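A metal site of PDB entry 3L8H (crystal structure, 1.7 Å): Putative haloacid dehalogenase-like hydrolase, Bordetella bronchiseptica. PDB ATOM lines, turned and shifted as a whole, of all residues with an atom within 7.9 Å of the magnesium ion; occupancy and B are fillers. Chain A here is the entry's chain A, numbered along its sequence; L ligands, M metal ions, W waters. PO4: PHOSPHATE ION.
The side-chain carboxylate (OD1) of Asp 7 is in salt-bridge range of the side-chain amino group (NZ) of Lys 101 (3.3 Å). N of Asp 7 sits at hydrogen-bond distance from O of Val 124 (2.9 Å). The side-chain carboxylate of Asp 9 lies within salt-bridge range of the guanidinium group of Arg 8 (2.7 Å). ND2 of Asn 13 lies within hydrogen-bond range of OD1 of Asp 9 (2.9 Å). N of Asp 126 lies within hydrogen-bond range of OD2 of Asp 130 (3.1 Å). The backbone NH (N) of Asn 148 is in hydrogen-bond range of the side-chain carboxylate (OD2) of Asp 126, 2.9 Å away. The backbone NH (N) of Gly 149 sits at hydrogen-bond distance from the backbone carbonyl oxygen (O) of Asp 126, 3.1 Å away. The side-chain carboxylate of Asp 130 lies within hydrogen-bond range of the backbone NH of Ser 127 (2.9 Å).
Asp 130 touches the magnesium ion. Of the 25 residues printed, 4 come within 4 Å of the magnesium ion.
OD2 of Asp 7 binds the magnesium ion, at 2.1 Å. The magnesium ion is bound by O1 of the ligand (2.1 Å). O of Asp 9 is bound to the magnesium ion (2.2 Å). Water W2 binds the magnesium ion. The magnesium ion is bound by water W1 (2.2 Å). OD1 of Asp 126 is bound to the magnesium ion, 2.2 Å away.
Water W1 lies within hydrogen-bond range of the side-chain carboxylate of Asp 130 (2.6 Å) and the side-chain hydroxyl of Ser 127 (2.8 Å).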
ATOM      1  N   LEU A   6     -20.495   0.381 -15.035  1.00  0.00           N
ATOM      2  CA  LEU A   6     -21.019   1.547 -14.323  1.00  0.00           C
ATOM      3  C   LEU A   6     -20.517   2.832 -14.932  1.00  0.00           C
ATOM      4  O   LEU A   6     -19.339   2.966 -15.253  1.00  0.00           O
ATOM      5  CB  LEU A   6     -20.551   1.538 -12.864  1.00  0.00           C
ATOM      6  CG  LEU A   6     -20.762   0.272 -12.053  1.00  0.00           C
ATOM      7  CD1 LEU A   6     -20.138   0.464 -10.662  1.00  0.00           C
ATOM      8  CD2 LEU A   6     -22.256  -0.038 -11.957  1.00  0.00           C
ATOM      9  N   ASP A   7     -21.411   3.800 -15.042  1.00  0.00           N
ATOM     10  CA  ASP A   7     -20.991   5.169 -15.256  1.00  0.00           C
ATOM     11  C   ASP A   7     -20.364   5.656 -13.962  1.00  0.00           C
ATOM     12  O   ASP A   7     -20.573   5.042 -12.904  1.00  0.00           O
ATOM     13  CB  ASP A   7     -22.218   6.005 -15.600  1.00  0.00           C
ATOM     14  CG  ASP A   7     -21.860   7.402 -15.998  1.00  0.00           C
ATOM     15  OD1 ASP A   7     -20.927   7.576 -16.816  1.00  0.00           O
ATOM     16  OD2 ASP A   7     -22.488   8.314 -15.467  1.00  0.00           O
ATOM     17  N   ARG A   8     -19.587   6.738 -14.016  1.00  0.00           N
ATOM     18  CA  ARG A   8     -18.923   7.241 -12.816  1.00  0.00           C
ATOM     19  C   ARG A   8     -19.656   8.422 -12.158  1.00  0.00           C
ATOM     20  O   ARG A   8     -20.295   8.237 -11.138  1.00  0.00           O
ATOM     21  CB  ARG A   8     -17.450   7.569 -13.056  1.00  0.00           C
ATOM     22  CG  ARG A   8     -16.619   7.583 -11.773  1.00  0.00           C
ATOM     23  CD  ARG A   8     -15.313   8.371 -11.931  1.00  0.00           C
ATOM     24  NE  ARG A   8     -15.592   9.796 -11.891  1.00  0.00           N
ATOM     25  CZ  ARG A   8     -14.705  10.751 -12.139  1.00  0.00           C
ATOM     26  NH1 ARG A   8     -13.453  10.417 -12.461  1.00  0.00           N
ATOM     27  NH2 ARG A   8     -15.053  12.046 -12.069  1.00  0.00           N
ATOM     28  N   ASP A   9     -19.587   9.613 -12.761  1.00  0.00           N
ATOM     29  CA  ASP A   9     -20.253  10.783 -12.187  1.00  0.00           C
ATOM     30  C   ASP A   9     -21.769  10.563 -12.106  1.00  0.00           C
ATOM     31  O   ASP A   9     -22.379  10.160 -13.075  1.00  0.00           O
ATOM     32  CB  ASP A   9     -19.975  12.055 -13.020  1.00  0.00           C
ATOM     33  CG  ASP A   9     -18.603  12.670 -12.771  1.00  0.00           C
ATOM     34  OD1 ASP A   9     -17.795  12.101 -12.013  1.00  0.00           O
ATOM     35  OD2 ASP A   9     -18.342  13.753 -13.326  1.00  0.00           O
ATOM     36  N   GLY A  10     -22.352  10.791 -10.935  1.00  0.00           N
ATOM     37  CA  GLY A  10     -23.788  10.617 -10.770  1.00  0.00           C
ATOM     38  C   GLY A  10     -24.234   9.216 -10.399  1.00  0.00           C
ATOM     39  O   GLY A  10     -25.418   9.001 -10.166  1.00  0.00           O
ATOM     40  N   VAL A  11     -23.293   8.261 -10.370  1.00  0.00           N
ATOM     41  CA  VAL A  11     -23.594   6.872 -10.031  1.00  0.00           C
ATOM     42  C   VAL A  11     -22.661   6.455  -8.870  1.00  0.00           C
ATOM     43  O   VAL A  11     -23.129   6.063  -7.791  1.00  0.00           O
ATOM     44  CB  VAL A  11     -23.424   5.937 -11.255  1.00  0.00           C
ATOM     45  CG1 VAL A  11     -23.649   4.485 -10.851  1.00  0.00           C
ATOM     46  CG2 VAL A  11     -24.412   6.328 -12.397  1.00  0.00           C
ATOM     47  N   VAL A  12     -21.348   6.540  -9.104  1.00  0.00           N
ATOM     48  CA  VAL A  12     -20.372   6.233  -8.045  1.00  0.00           C
ATOM     49  C   VAL A  12     -20.143   7.447  -7.154  1.00  0.00           C
ATOM     50  O   VAL A  12     -20.197   7.351  -5.921  1.00  0.00           O
ATOM     51  CB  VAL A  12     -19.050   5.732  -8.631  1.00  0.00           C
ATOM     52  CG1 VAL A  12     -18.100   5.304  -7.492  1.00  0.00           C
ATOM     53  CG2 VAL A  12     -19.303   4.551  -9.594  1.00  0.00           C
ATOM     54  N   ASN A  13     -19.884   8.595  -7.774  1.00  0.00           N
ATOM     55  CA  ASN A  13     -19.597   9.818  -7.040  1.00  0.00           C
ATOM     56  C   ASN A  13     -20.560  10.922  -7.439  1.00  0.00           C
ATOM     57  O   ASN A  13     -21.224  10.823  -8.475  1.00  0.00           O
ATOM     58  CB  ASN A  13     -18.178  10.294  -7.284  1.00  0.00           C
ATOM     59  CG  ASN A  13     -17.899  10.548  -8.735  1.00  0.00           C
ATOM     60  OD1 ASN A  13     -17.752   9.608  -9.525  1.00  0.00           O
ATOM     61  ND2 ASN A  13     -17.825  11.822  -9.116  1.00  0.00           N
ATOM     62  N   ASP A  15     -22.209  14.026  -9.005  1.00  0.00           N
ATOM     63  CA  ASP A  15     -21.971  14.852 -10.184  1.00  0.00           C
ATOM     64  C   ASP A  15     -21.692  16.298  -9.756  1.00  0.00           C
ATOM     65  O   ASP A  15     -22.045  16.728  -8.653  1.00  0.00           O
ATOM     66  CB  ASP A  15     -23.159  14.808 -11.150  1.00  0.00           C
ATOM     67  CG  ASP A  15     -24.411  15.461 -10.563  1.00  0.00           C
ATOM     68  OD1 ASP A  15     -24.946  14.955  -9.557  1.00  0.00           O
ATOM     69  OD2 ASP A  15     -24.875  16.470 -11.144  1.00  0.00           O
ATOM     70  N   ALA A  49     -17.353   2.985 -17.257  1.00  0.00           N
ATOM     71  CA  ALA A  49     -17.339   3.577 -18.600  1.00  0.00           C
ATOM     72  C   ALA A  49     -17.790   4.991 -18.382  1.00  0.00           C
ATOM     73  O   ALA A  49     -18.961   5.229 -18.084  1.00  0.00           O
ATOM     74  CB  ALA A  49     -18.289   2.850 -19.513  1.00  0.00           C
ATOM     75  N   THR A  50     -16.864   5.932 -18.535  1.00  0.00           N
ATOM     76  CA  THR A  50     -17.143   7.317 -18.123  1.00  0.00           C
ATOM     77  C   THR A  50     -16.731   8.358 -19.183  1.00  0.00           C
ATOM     78  O   THR A  50     -15.643   8.271 -19.735  1.00  0.00           O
ATOM     79  CB  THR A  50     -16.466   7.618 -16.752  1.00  0.00           C
ATOM     80  OG1 THR A  50     -16.626   8.994 -16.421  1.00  0.00           O
ATOM     81  CG2 THR A  50     -14.955   7.278 -16.770  1.00  0.00           C
ATOM     82  N   ASN A  51     -17.614   9.321 -19.436  1.00  0.00           N
ATOM     83  CA  ASN A  51     -17.245  10.497 -20.235  1.00  0.00           C
ATOM     84  C   ASN A  51     -16.443  11.448 -19.346  1.00  0.00           C
ATOM     85  O   ASN A  51     -16.915  11.847 -18.279  1.00  0.00           O
ATOM     86  CB  ASN A  51     -18.504  11.232 -20.738  1.00  0.00           C
ATOM     87  CG  ASN A  51     -19.107  10.623 -22.015  1.00  0.00           C
ATOM     88  OD1 ASN A  51     -18.612   9.646 -22.576  1.00  0.00           O
ATOM     89  ND2 ASN A  51     -20.215  11.209 -22.464  1.00  0.00           N
ATOM     90  N   GLN A  52     -15.239  11.824 -19.789  1.00  0.00           N
ATOM     91  CA  GLN A  52     -14.369  12.729 -19.020  1.00  0.00           C
ATOM     92  C   GLN A  52     -13.872  13.895 -19.886  1.00  0.00           C
ATOM     93  O   GLN A  52     -12.676  14.057 -20.136  1.00  0.00           O
ATOM     94  CB  GLN A  52     -13.188  11.937 -18.418  1.00  0.00           C
ATOM     95  CG  GLN A  52     -13.648  11.002 -17.321  1.00  0.00           C
ATOM     96  CD  GLN A  52     -14.111  11.766 -16.101  1.00  0.00           C
ATOM     97  OE1 GLN A  52     -13.489  12.760 -15.724  1.00  0.00           O
ATOM     98  NE2 GLN A  52     -15.209  11.320 -15.477  1.00  0.00           N
ATOM     99  N   LYS A 101     -20.238   8.717 -25.054  1.00  0.00           N
ATOM    100  CA  LYS A 101     -21.643   8.360 -24.960  1.00  0.00           C
ATOM    101  C   LYS A 101     -22.470   9.551 -25.465  1.00  0.00           C
ATOM    102  O   LYS A 101     -22.143  10.681 -25.132  1.00  0.00           O
ATOM    103  CB  LYS A 101     -22.010   8.053 -23.499  1.00  0.00           C
ATOM    104  CG  LYS A 101     -21.075   7.053 -22.824  1.00  0.00           C
ATOM    105  CD  LYS A 101     -21.695   6.644 -21.485  1.00  0.00           C
ATOM    106  CE  LYS A 101     -20.710   6.053 -20.530  1.00  0.00           C
ATOM    107  NZ  LYS A 101     -21.454   5.480 -19.366  1.00  0.00           N
ATOM    108  N   VAL A 124     -25.175   0.520 -15.591  1.00  0.00           N
ATOM    109  CA  VAL A 124     -25.843   1.485 -14.730  1.00  0.00           C
ATOM    110  C   VAL A 124     -25.436   2.903 -15.062  1.00  0.00           C
ATOM    111  O   VAL A 124     -24.243   3.203 -15.127  1.00  0.00           O
ATOM    112  CB  VAL A 124     -25.491   1.191 -13.246  1.00  0.00           C
ATOM    113  CG1 VAL A 124     -26.284   2.103 -12.331  1.00  0.00           C
ATOM    114  CG2 VAL A 124     -25.769  -0.269 -12.927  1.00  0.00           C
ATOM    115  N   GLY A 125     -26.404   3.780 -15.272  1.00  0.00           N
ATOM    116  CA  GLY A 125     -26.116   5.168 -15.594  1.00  0.00           C
ATOM    117  C   GLY A 125     -27.103   6.127 -14.970  1.00  0.00           C
ATOM    118  O   GLY A 125     -28.164   5.712 -14.468  1.00  0.00           O
ATOM    119  N   ASP A 126     -26.764   7.421 -14.980  1.00  0.00           N
ATOM    120  CA  ASP A 126     -27.674   8.434 -14.470  1.00  0.00           C
ATOM    121  C   ASP A 126     -28.185   9.364 -15.558  1.00  0.00           C
ATOM    122  O   ASP A 126     -29.017  10.222 -15.272  1.00  0.00           O
ATOM    123  CB  ASP A 126     -27.037   9.260 -13.354  1.00  0.00           C
ATOM    124  CG  ASP A 126     -25.886  10.132 -13.846  1.00  0.00           C
ATOM    125  OD1 ASP A 126     -25.007   9.608 -14.557  1.00  0.00           O
ATOM    126  OD2 ASP A 126     -25.823  11.323 -13.487  1.00  0.00           O
ATOM    127  N   SER A 127     -27.660   9.209 -16.762  1.00  0.00           N
ATOM    128  CA  SER A 127     -28.014  10.083 -17.894  1.00  0.00           C
ATOM    129  C   SER A 127     -28.569   9.301 -19.069  1.00  0.00           C
ATOM    130  O   SER A 127     -28.216   8.147 -19.294  1.00  0.00           O
ATOM    131  CB  SER A 127     -26.793  10.846 -18.351  1.00  0.00           C
ATOM    132  OG  SER A 127     -26.292  11.652 -17.316  1.00  0.00           O
ATOM    133  N   ARG A 129     -27.784   9.431 -22.105  1.00  0.00           N
ATOM    134  CA  ARG A 129     -26.725   8.966 -22.996  1.00  0.00           C
ATOM    135  C   ARG A 129     -26.066   7.676 -22.489  1.00  0.00           C
ATOM    136  O   ARG A 129     -25.591   6.871 -23.278  1.00  0.00           O
ATOM    137  CB  ARG A 129     -25.669  10.055 -23.234  1.00  0.00           C
ATOM    138  CG  ARG A 129     -24.847  10.436 -22.013  1.00  0.00           C
ATOM    139  CD  ARG A 129     -23.839  11.561 -22.327  1.00  0.00           C
ATOM    140  NE  ARG A 129     -24.526  12.835 -22.584  1.00  0.00           N
ATOM    141  CZ  ARG A 129     -24.377  13.572 -23.690  1.00  0.00           C
ATOM    142  NH1 ARG A 129     -23.573  13.176 -24.672  1.00  0.00           N
ATOM    143  NH2 ARG A 129     -25.052  14.710 -23.817  1.00  0.00           N
ATOM    144  N   ASP A 130     -26.066   7.468 -21.173  1.00  0.00           N
ATOM    145  CA  ASP A 130     -25.524   6.239 -20.609  1.00  0.00           C
ATOM    146  C   ASP A 130     -26.401   5.073 -21.036  1.00  0.00           C
ATOM    147  O   ASP A 130     -25.909   4.009 -21.420  1.00  0.00           O
ATOM    148  CB  ASP A 130     -25.527   6.274 -19.080  1.00  0.00           C
ATOM    149  CG  ASP A 130     -24.657   7.366 -18.494  1.00  0.00           C
ATOM    150  OD1 ASP A 130     -23.540   7.598 -19.028  1.00  0.00           O
ATOM    151  OD2 ASP A 130     -25.092   7.989 -17.486  1.00  0.00           O
ATOM    152  N   VAL A 144     -30.181   5.028 -12.349  1.00  0.00           N
ATOM    153  CA  VAL A 144     -30.280   5.478 -10.955  1.00  0.00           C
ATOM    154  C   VAL A 144     -30.906   6.864 -10.897  1.00  0.00           C
ATOM    155  O   VAL A 144     -30.972   7.559 -11.903  1.00  0.00           O
ATOM    156  CB  VAL A 144     -28.927   5.455 -10.212  1.00  0.00           C
ATOM    157  CG1 VAL A 144     -28.438   4.001 -10.058  1.00  0.00           C
ATOM    158  CG2 VAL A 144     -27.863   6.301 -10.904  1.00  0.00           C
ATOM    159  N   THR A 146     -29.899   9.235  -8.537  1.00  0.00           N
ATOM    160  CA  THR A 146     -28.841  10.204  -8.221  1.00  0.00           C
ATOM    161  C   THR A 146     -28.365  10.915  -9.487  1.00  0.00           C
ATOM    162  O   THR A 146     -28.734  10.518 -10.596  1.00  0.00           O
ATOM    163  CB  THR A 146     -27.668   9.491  -7.513  1.00  0.00           C
ATOM    164  OG1 THR A 146     -27.233   8.386  -8.317  1.00  0.00           O
ATOM    165  CG2 THR A 146     -28.144   8.974  -6.185  1.00  0.00           C
ATOM    166  N   GLY A 147     -27.554  11.962  -9.335  1.00  0.00           N
ATOM    167  CA  GLY A 147     -27.032  12.653 -10.506  1.00  0.00           C
ATOM    168  C   GLY A 147     -28.148  13.201 -11.371  1.00  0.00           C
ATOM    169  O   GLY A 147     -29.104  13.802 -10.863  1.00  0.00           O
ATOM    170  N   ASN A 148     -28.050  12.941 -12.670  1.00  0.00           N
ATOM    171  CA  ASN A 148     -29.052  13.405 -13.622  1.00  0.00           C
ATOM    172  C   ASN A 148     -30.268  12.478 -13.702  1.00  0.00           C
ATOM    173  O   ASN A 148     -31.118  12.657 -14.552  1.00  0.00           O
ATOM    174  CB  ASN A 148     -28.432  13.518 -15.029  1.00  0.00           C
ATOM    175  CG  ASN A 148     -27.395  14.602 -15.119  1.00  0.00           C
ATOM    176  OD1 ASN A 148     -27.548  15.667 -14.515  1.00  0.00           O
ATOM    177  ND2 ASN A 148     -26.330  14.356 -15.882  1.00  0.00           N
ATOM    178  N   GLY A 149     -30.347  11.488 -12.804  1.00  0.00           N
ATOM    179  CA  GLY A 149     -31.312  10.412 -13.001  1.00  0.00           C
ATOM    180  C   GLY A 149     -32.777  10.820 -12.900  1.00  0.00           C
ATOM    181  O   GLY A 149     -33.627  10.307 -13.625  1.00  0.00           O
HETATM  182  P   PO4 L   1     -19.838  10.496 -16.483  1.00  0.00           P
HETATM  183  O1  PO4 L   1     -21.176  10.974 -15.932  1.00  0.00           O
HETATM  184  O2  PO4 L   1     -20.057   9.634 -17.714  1.00  0.00           O
HETATM  185  O3  PO4 L   1     -19.021  11.710 -16.907  1.00  0.00           O
HETATM  186  O4  PO4 L   1     -19.010   9.718 -15.456  1.00  0.00           O
HETATM  187 MG    MG M   1     -22.995  10.308 -15.133  1.00  0.00          MG
HETATM  188  O   HOH W   1     -23.875  10.311 -17.111  1.00  0.00           O
HETATM  189  O   HOH W   2     -23.646  12.343 -14.791  1.00  0.00           O
